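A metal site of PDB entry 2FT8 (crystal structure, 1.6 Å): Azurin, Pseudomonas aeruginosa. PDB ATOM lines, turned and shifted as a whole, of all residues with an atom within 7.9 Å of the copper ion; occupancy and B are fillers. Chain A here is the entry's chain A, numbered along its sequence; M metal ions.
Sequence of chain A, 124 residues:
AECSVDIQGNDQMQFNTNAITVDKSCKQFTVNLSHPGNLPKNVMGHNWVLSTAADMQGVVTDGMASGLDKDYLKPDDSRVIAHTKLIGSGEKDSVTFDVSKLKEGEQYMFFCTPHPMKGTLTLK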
ATOM      1  N   GLY A   9      -8.157  13.181   8.714  1.00  0.00           N
ATOM      2  CA  GLY A   9      -8.144  14.209   7.678  1.00  0.00           C
ATOM      3  C   GLY A   9      -9.419  15.017   7.812  1.00  0.00           C
ATOM      4  O   GLY A   9     -10.508  14.453   7.950  1.00  0.00           O
ATOM      5  N   ASN A  10      -9.273  16.338   7.777  1.00  0.00           N
ATOM      6  CA  ASN A  10     -10.410  17.214   8.116  1.00  0.00           C
ATOM      7  C   ASN A  10     -10.916  17.997   6.907  1.00  0.00           C
ATOM      8  O   ASN A  10     -10.507  17.798   5.793  1.00  0.00           O
ATOM      9  CB  ASN A  10     -10.055  18.088   9.307  1.00  0.00           C
ATOM     10  CG  ASN A  10      -9.040  19.137   8.996  1.00  0.00           C
ATOM     11  OD1 ASN A  10      -8.645  19.339   7.822  1.00  0.00           O
ATOM     12  ND2 ASN A  10      -8.558  19.816  10.044  1.00  0.00           N
ATOM     13  N   MET A  13      -8.378  20.058   4.573  1.00  0.00           N
ATOM     14  CA  MET A  13      -7.324  19.339   3.841  1.00  0.00           C
ATOM     15  C   MET A  13      -6.053  19.247   4.692  1.00  0.00           C
ATOM     16  O   MET A  13      -4.945  19.503   4.205  1.00  0.00           O
ATOM     17  CB  MET A  13      -7.037  20.061   2.505  1.00  0.00           C
ATOM     18  CG  MET A  13      -8.121  20.098   1.511  1.00  0.00           C
ATOM     19  SD  MET A  13      -7.492  20.729  -0.084  1.00  0.00           S
ATOM     20  CE  MET A  13      -6.605  22.199   0.446  1.00  0.00           C
ATOM     21  N   GLN A  14      -6.219  18.876   5.957  1.00  0.00           N
ATOM     22  CA  GLN A  14      -5.105  18.667   6.840  1.00  0.00           C
ATOM     23  C   GLN A  14      -5.159  17.278   7.450  1.00  0.00           C
ATOM     24  O   GLN A  14      -6.208  16.895   7.981  1.00  0.00           O
ATOM     25  CB  GLN A  14      -5.151  19.639   8.021  1.00  0.00           C
ATOM     26  CG  GLN A  14      -5.027  21.090   7.557  1.00  0.00           C
ATOM     27  CD  GLN A  14      -5.419  22.113   8.596  1.00  0.00           C
ATOM     28  OE1 GLN A  14      -6.148  21.815   9.557  1.00  0.00           O
ATOM     29  NE2 GLN A  14      -4.921  23.328   8.409  1.00  0.00           N
ATOM     30  N   PHE A  15      -4.042  16.561   7.407  1.00  0.00           N
ATOM     31  CA  PHE A  15      -3.886  15.363   8.254  1.00  0.00           C
ATOM     32  C   PHE A  15      -3.484  15.861   9.647  1.00  0.00           C
ATOM     33  O   PHE A  15      -2.820  16.923   9.765  1.00  0.00           O
ATOM     34  CB  PHE A  15      -2.769  14.451   7.739  1.00  0.00           C
ATOM     35  CG  PHE A  15      -3.142  13.578   6.573  1.00  0.00           C
ATOM     36  CD1 PHE A  15      -4.237  12.776   6.613  1.00  0.00           C
ATOM     37  CD2 PHE A  15      -2.320  13.487   5.457  1.00  0.00           C
ATOM     38  CE1 PHE A  15      -4.553  11.919   5.588  1.00  0.00           C
ATOM     39  CE2 PHE A  15      -2.639  12.642   4.384  1.00  0.00           C
ATOM     40  CZ  PHE A  15      -3.750  11.868   4.444  1.00  0.00           C
ATOM     41  N   LEU A  33      -7.883   5.484   9.545  1.00  0.00           N
ATOM     42  CA  LEU A  33      -8.200   6.811   8.999  1.00  0.00           C
ATOM     43  C   LEU A  33      -9.626   7.199   9.351  1.00  0.00           C
ATOM     44  O   LEU A  33     -10.568   6.399   9.221  1.00  0.00           O
ATOM     45  CB  LEU A  33      -8.028   6.814   7.473  1.00  0.00           C
ATOM     46  CG  LEU A  33      -8.223   8.160   6.761  1.00  0.00           C
ATOM     47  CD1 LEU A  33      -7.139   9.186   7.159  1.00  0.00           C
ATOM     48  CD2 LEU A  33      -8.273   7.984   5.255  1.00  0.00           C
ATOM     49  N   HIS A  35     -12.312  11.089   9.642  1.00  0.00           N
ATOM     50  CA  HIS A  35     -12.576  12.375   8.928  1.00  0.00           C
ATOM     51  C   HIS A  35     -13.518  13.236   9.760  1.00  0.00           C
ATOM     52  O   HIS A  35     -14.714  13.324   9.472  1.00  0.00           O
ATOM     53  CB  HIS A  35     -13.139  12.102   7.537  1.00  0.00           C
ATOM     54  CG  HIS A  35     -13.261  13.305   6.624  1.00  0.00           C
ATOM     55  ND1 HIS A  35     -13.491  14.600   7.063  1.00  0.00           N
ATOM     56  CD2 HIS A  35     -13.279  13.346   5.266  1.00  0.00           C
ATOM     57  CE1 HIS A  35     -13.629  15.396   6.001  1.00  0.00           C
ATOM     58  NE2 HIS A  35     -13.492  14.665   4.897  1.00  0.00           N
ATOM     59  N   MET A  44     -15.007  16.342  -0.291  1.00  0.00           N
ATOM     60  CA  MET A  44     -13.834  16.498   0.559  1.00  0.00           C
ATOM     61  C   MET A  44     -13.473  15.102   1.073  1.00  0.00           C
ATOM     62  O   MET A  44     -13.279  14.890   2.280  1.00  0.00           O
ATOM     63  CB  MET A  44     -14.066  17.484   1.694  1.00  0.00           C
ATOM     64  CG  MET A  44     -12.878  17.821   2.583  1.00  0.00           C
ATOM     65  SD  MET A  44     -11.509  18.486   1.702  1.00  0.00           S
ATOM     66  CE  MET A  44     -12.184  20.058   1.137  1.00  0.00           C
ATOM     67  N   GLY A  45     -13.438  14.151   0.160  1.00  0.00           N
ATOM     68  CA  GLY A  45     -12.983  12.826   0.463  1.00  0.00           C
ATOM     69  C   GLY A  45     -11.485  12.751   0.627  1.00  0.00           C
ATOM     70  O   GLY A  45     -10.729  13.401  -0.100  1.00  0.00           O
ATOM     71  N   HIS A  46     -11.077  11.965   1.608  1.00  0.00           N
ATOM     72  CA  HIS A  46      -9.640  11.696   1.829  1.00  0.00           C
ATOM     73  C   HIS A  46      -9.343  10.224   1.749  1.00  0.00           C
ATOM     74  O   HIS A  46     -10.137   9.379   2.155  1.00  0.00           O
ATOM     75  CB  HIS A  46      -9.188  12.155   3.229  1.00  0.00           C
ATOM     76  CG  HIS A  46      -9.396  13.617   3.503  1.00  0.00           C
ATOM     77  ND1 HIS A  46      -9.010  14.607   2.617  1.00  0.00           N
ATOM     78  CD2 HIS A  46      -9.990  14.239   4.547  1.00  0.00           C
ATOM     79  CE1 HIS A  46      -9.327  15.790   3.137  1.00  0.00           C
ATOM     80  NE2 HIS A  46      -9.907  15.589   4.313  1.00  0.00           N
ATOM     81  N   ASN A  47      -8.160   9.911   1.245  1.00  0.00           N
ATOM     82  CA  ASN A  47      -7.595   8.557   1.390  1.00  0.00           C
ATOM     83  C   ASN A  47      -6.236   8.685   2.046  1.00  0.00           C
ATOM     84  O   ASN A  47      -5.733   9.792   2.276  1.00  0.00           O
ATOM     85  CB  ASN A  47      -7.580   7.745   0.057  1.00  0.00           C
ATOM     86  CG  ASN A  47      -6.846   8.480  -1.100  1.00  0.00           C
ATOM     87  OD1 ASN A  47      -5.984   9.342  -0.851  1.00  0.00           O
ATOM     88  ND2 ASN A  47      -7.207   8.134  -2.369  1.00  0.00           N
ATOM     89  N   TRP A  48      -5.687   7.522   2.435  1.00  0.00           N
ATOM     90  CA  TRP A  48      -4.354   7.460   3.005  1.00  0.00           C
ATOM     91  C   TRP A  48      -3.650   6.390   2.117  1.00  0.00           C
ATOM     92  O   TRP A  48      -4.099   5.241   2.052  1.00  0.00           O
ATOM     93  CB  TRP A  48      -4.394   7.040   4.467  1.00  0.00           C
ATOM     94  CG  TRP A  48      -3.025   6.996   5.136  1.00  0.00           C
ATOM     95  CD1 TRP A  48      -2.443   7.994   5.847  1.00  0.00           C
ATOM     96  CD2 TRP A  48      -2.076   5.898   5.108  1.00  0.00           C
ATOM     97  NE1 TRP A  48      -1.185   7.598   6.281  1.00  0.00           N
ATOM     98  CE2 TRP A  48      -0.944   6.318   5.853  1.00  0.00           C
ATOM     99  CE3 TRP A  48      -2.095   4.603   4.568  1.00  0.00           C
ATOM    100  CZ2 TRP A  48       0.154   5.492   6.040  1.00  0.00           C
ATOM    101  CZ3 TRP A  48      -0.962   3.786   4.744  1.00  0.00           C
ATOM    102  CH2 TRP A  48       0.134   4.245   5.487  1.00  0.00           C
ATOM    103  N   TYR A  72      -9.903   7.518  -6.374  1.00  0.00           N
ATOM    104  CA  TYR A  72      -8.781   8.288  -6.894  1.00  0.00           C
ATOM    105  C   TYR A  72      -7.475   7.557  -6.823  1.00  0.00           C
ATOM    106  O   TYR A  72      -6.437   8.157  -6.537  1.00  0.00           O
ATOM    107  CB  TYR A  72      -8.660   9.647  -6.250  1.00  0.00           C
ATOM    108  CG  TYR A  72      -9.833  10.591  -6.496  1.00  0.00           C
ATOM    109  CD1 TYR A  72     -10.126  11.034  -7.778  1.00  0.00           C
ATOM    110  CD2 TYR A  72     -10.552  11.109  -5.444  1.00  0.00           C
ATOM    111  CE1 TYR A  72     -11.164  11.920  -8.000  1.00  0.00           C
ATOM    112  CE2 TYR A  72     -11.618  11.992  -5.655  1.00  0.00           C
ATOM    113  CZ  TYR A  72     -11.890  12.399  -6.930  1.00  0.00           C
ATOM    114  OH  TYR A  72     -12.934  13.318  -7.140  1.00  0.00           O
ATOM    115  N   LEU A  86     -11.484   5.992  -0.115  1.00  0.00           N
ATOM    116  CA  LEU A  86     -11.795   7.406   0.128  1.00  0.00           C
ATOM    117  C   LEU A  86     -12.917   7.446   1.156  1.00  0.00           C
ATOM    118  O   LEU A  86     -13.868   6.645   1.088  1.00  0.00           O
ATOM    119  CB  LEU A  86     -12.281   8.056  -1.184  1.00  0.00           C
ATOM    120  CG  LEU A  86     -12.128   9.564  -1.329  1.00  0.00           C
ATOM    121  CD1 LEU A  86     -10.654   9.854  -1.608  1.00  0.00           C
ATOM    122  CD2 LEU A  86     -13.053  10.087  -2.467  1.00  0.00           C
ATOM    123  N   ILE A  87     -12.789   8.367   2.099  1.00  0.00           N
ATOM    124  CA  ILE A  87     -13.825   8.555   3.104  1.00  0.00           C
ATOM    125  C   ILE A  87     -14.274  10.011   3.181  1.00  0.00           C
ATOM    126  O   ILE A  87     -13.468  10.923   3.063  1.00  0.00           O
ATOM    127  CB  ILE A  87     -13.379   8.060   4.516  1.00  0.00           C
ATOM    128  CG1 ILE A  87     -12.189   8.854   5.027  1.00  0.00           C
ATOM    129  CG2 ILE A  87     -13.107   6.585   4.516  1.00  0.00           C
ATOM    130  CD1 ILE A  87     -11.870   8.602   6.471  1.00  0.00           C
ATOM    131  N   PHE A 111       0.139   9.927   1.757  1.00  0.00           N
ATOM    132  CA  PHE A 111      -0.529  11.054   1.117  1.00  0.00           C
ATOM    133  C   PHE A 111      -1.974  10.709   0.801  1.00  0.00           C
ATOM    134  O   PHE A 111      -2.333   9.566   0.738  1.00  0.00           O
ATOM    135  CB  PHE A 111       0.220  11.474  -0.155  1.00  0.00           C
ATOM    136  CG  PHE A 111       0.563  10.335  -1.074  1.00  0.00           C
ATOM    137  CD1 PHE A 111       1.728   9.598  -0.882  1.00  0.00           C
ATOM    138  CD2 PHE A 111      -0.224  10.023  -2.160  1.00  0.00           C
ATOM    139  CE1 PHE A 111       2.083   8.549  -1.718  1.00  0.00           C
ATOM    140  CE2 PHE A 111       0.110   8.966  -3.003  1.00  0.00           C
ATOM    141  CZ  PHE A 111       1.264   8.247  -2.764  1.00  0.00           C
ATOM    142  N   CYS A 112      -2.761  11.774   0.638  1.00  0.00           N
ATOM    143  CA  CYS A 112      -4.082  11.723   0.056  1.00  0.00           C
ATOM    144  C   CYS A 112      -3.925  12.015  -1.448  1.00  0.00           C
ATOM    145  O   CYS A 112      -3.238  12.961  -1.800  1.00  0.00           O
ATOM    146  CB  CYS A 112      -4.926  12.795   0.688  1.00  0.00           C
ATOM    147  SG  CYS A 112      -6.579  12.897  -0.034  1.00  0.00           S
ATOM    148  N   THR A 113      -4.519  11.231  -2.316  1.00  0.00           N
ATOM    149  CA  THR A 113      -4.336  11.516  -3.774  1.00  0.00           C
ATOM    150  C   THR A 113      -5.043  12.794  -4.301  1.00  0.00           C
ATOM    151  O   THR A 113      -4.405  13.566  -5.019  1.00  0.00           O
ATOM    152  CB  THR A 113      -4.559  10.308  -4.674  1.00  0.00           C
ATOM    153  OG1 THR A 113      -5.843   9.776  -4.468  1.00  0.00           O
ATOM    154  CG2 THR A 113      -3.488   9.229  -4.458  1.00  0.00           C
ATOM    155  N   PRO A 114      -6.326  13.048  -3.946  1.00  0.00           N
ATOM    156  CA  PRO A 114      -6.920  14.299  -4.486  1.00  0.00           C
ATOM    157  C   PRO A 114      -6.402  15.601  -3.877  1.00  0.00           C
ATOM    158  O   PRO A 114      -6.581  16.656  -4.521  1.00  0.00           O
ATOM    159  CB  PRO A 114      -8.420  14.129  -4.236  1.00  0.00           C
ATOM    160  CG  PRO A 114      -8.509  13.135  -3.107  1.00  0.00           C
ATOM    161  CD  PRO A 114      -7.318  12.215  -3.258  1.00  0.00           C
ATOM    162  N   HIS A 115      -5.827  15.603  -2.668  1.00  0.00           N
ATOM    163  CA  HIS A 115      -5.538  16.847  -1.949  1.00  0.00           C
ATOM    164  C   HIS A 115      -4.084  16.951  -1.637  1.00  0.00           C
ATOM    165  O   HIS A 115      -3.388  15.919  -1.530  1.00  0.00           O
ATOM    166  CB  HIS A 115      -6.359  16.948  -0.648  1.00  0.00           C
ATOM    167  CG  HIS A 115      -7.834  16.925  -0.889  1.00  0.00           C
ATOM    168  ND1 HIS A 115      -8.684  16.039  -0.252  1.00  0.00           N
ATOM    169  CD2 HIS A 115      -8.615  17.689  -1.685  1.00  0.00           C
ATOM    170  CE1 HIS A 115      -9.908  16.213  -0.695  1.00  0.00           C
ATOM    171  NE2 HIS A 115      -9.904  17.219  -1.562  1.00  0.00           N
ATOM    172  N   PRO A 116      -3.579  18.176  -1.502  1.00  0.00           N
ATOM    173  CA  PRO A 116      -2.186  18.450  -1.134  1.00  0.00           C
ATOM    174  C   PRO A 116      -1.931  18.184   0.354  1.00  0.00           C
ATOM    175  O   PRO A 116      -1.713  19.081   1.152  1.00  0.00           O
ATOM    176  CB  PRO A 116      -2.009  19.951  -1.544  1.00  0.00           C
ATOM    177  CG  PRO A 116      -3.348  20.490  -1.404  1.00  0.00           C
ATOM    178  CD  PRO A 116      -4.315  19.439  -1.771  1.00  0.00           C
ATOM    179  N   MET A 117      -1.955  16.897   0.707  1.00  0.00           N
ATOM    180  CA  MET A 117      -1.763  16.438   2.085  1.00  0.00           C
ATOM    181  C   MET A 117      -0.784  15.262   2.077  1.00  0.00           C
ATOM    182  O   MET A 117      -0.999  14.301   1.385  1.00  0.00           O
ATOM    183  CB  MET A 117      -3.089  15.897   2.675  1.00  0.00           C
ATOM    184  CG  MET A 117      -4.163  16.911   2.839  1.00  0.00           C
ATOM    185  SD  MET A 117      -5.827  16.146   2.815  1.00  0.00           S
ATOM    186  CE  MET A 117      -5.818  15.205   4.304  1.00  0.00           C
HETATM  187 CU    CU M   1      -7.771  14.410   0.967  1.00  0.00          CU
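N of Cys 112 lies within hydrogen-bond range of O of Met 117 (3.2 Å). The backbone carbonyl oxygen of Asn 10 is in hydrogen-bond range of a ring nitrogen (NE2) of His 46. A ring nitrogen (ND1) of His 115 sits close to the backbone carbonyl oxygen of Gly 45, 3.3 Å away. N of Ile 87 sits at hydrogen-bond distance from O of His 46, 2.8 Å away. The side-chain sulfur (SD) of Met 117 sits close to a ring nitrogen (ND1) of His 46 (3.5 Å). The backbone NH of Asn 47 sits close to the side-chain sulfur of Cys 112, 3.6 Å away.
Residues that only touch the copper ion: Gly 45 and Met 117. Of the 22 residues printed, 5 come within 4 Å of the copper ion.
The copper ion is bound by a ring nitrogen (ND1) of His 46 (2.1 Å), the side-chain sulfur of Cys 112 (2.2 Å) and a ring nitrogen (ND1) of His 115 (2.2 Å). The copper ion has three donor atoms within binding distance.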
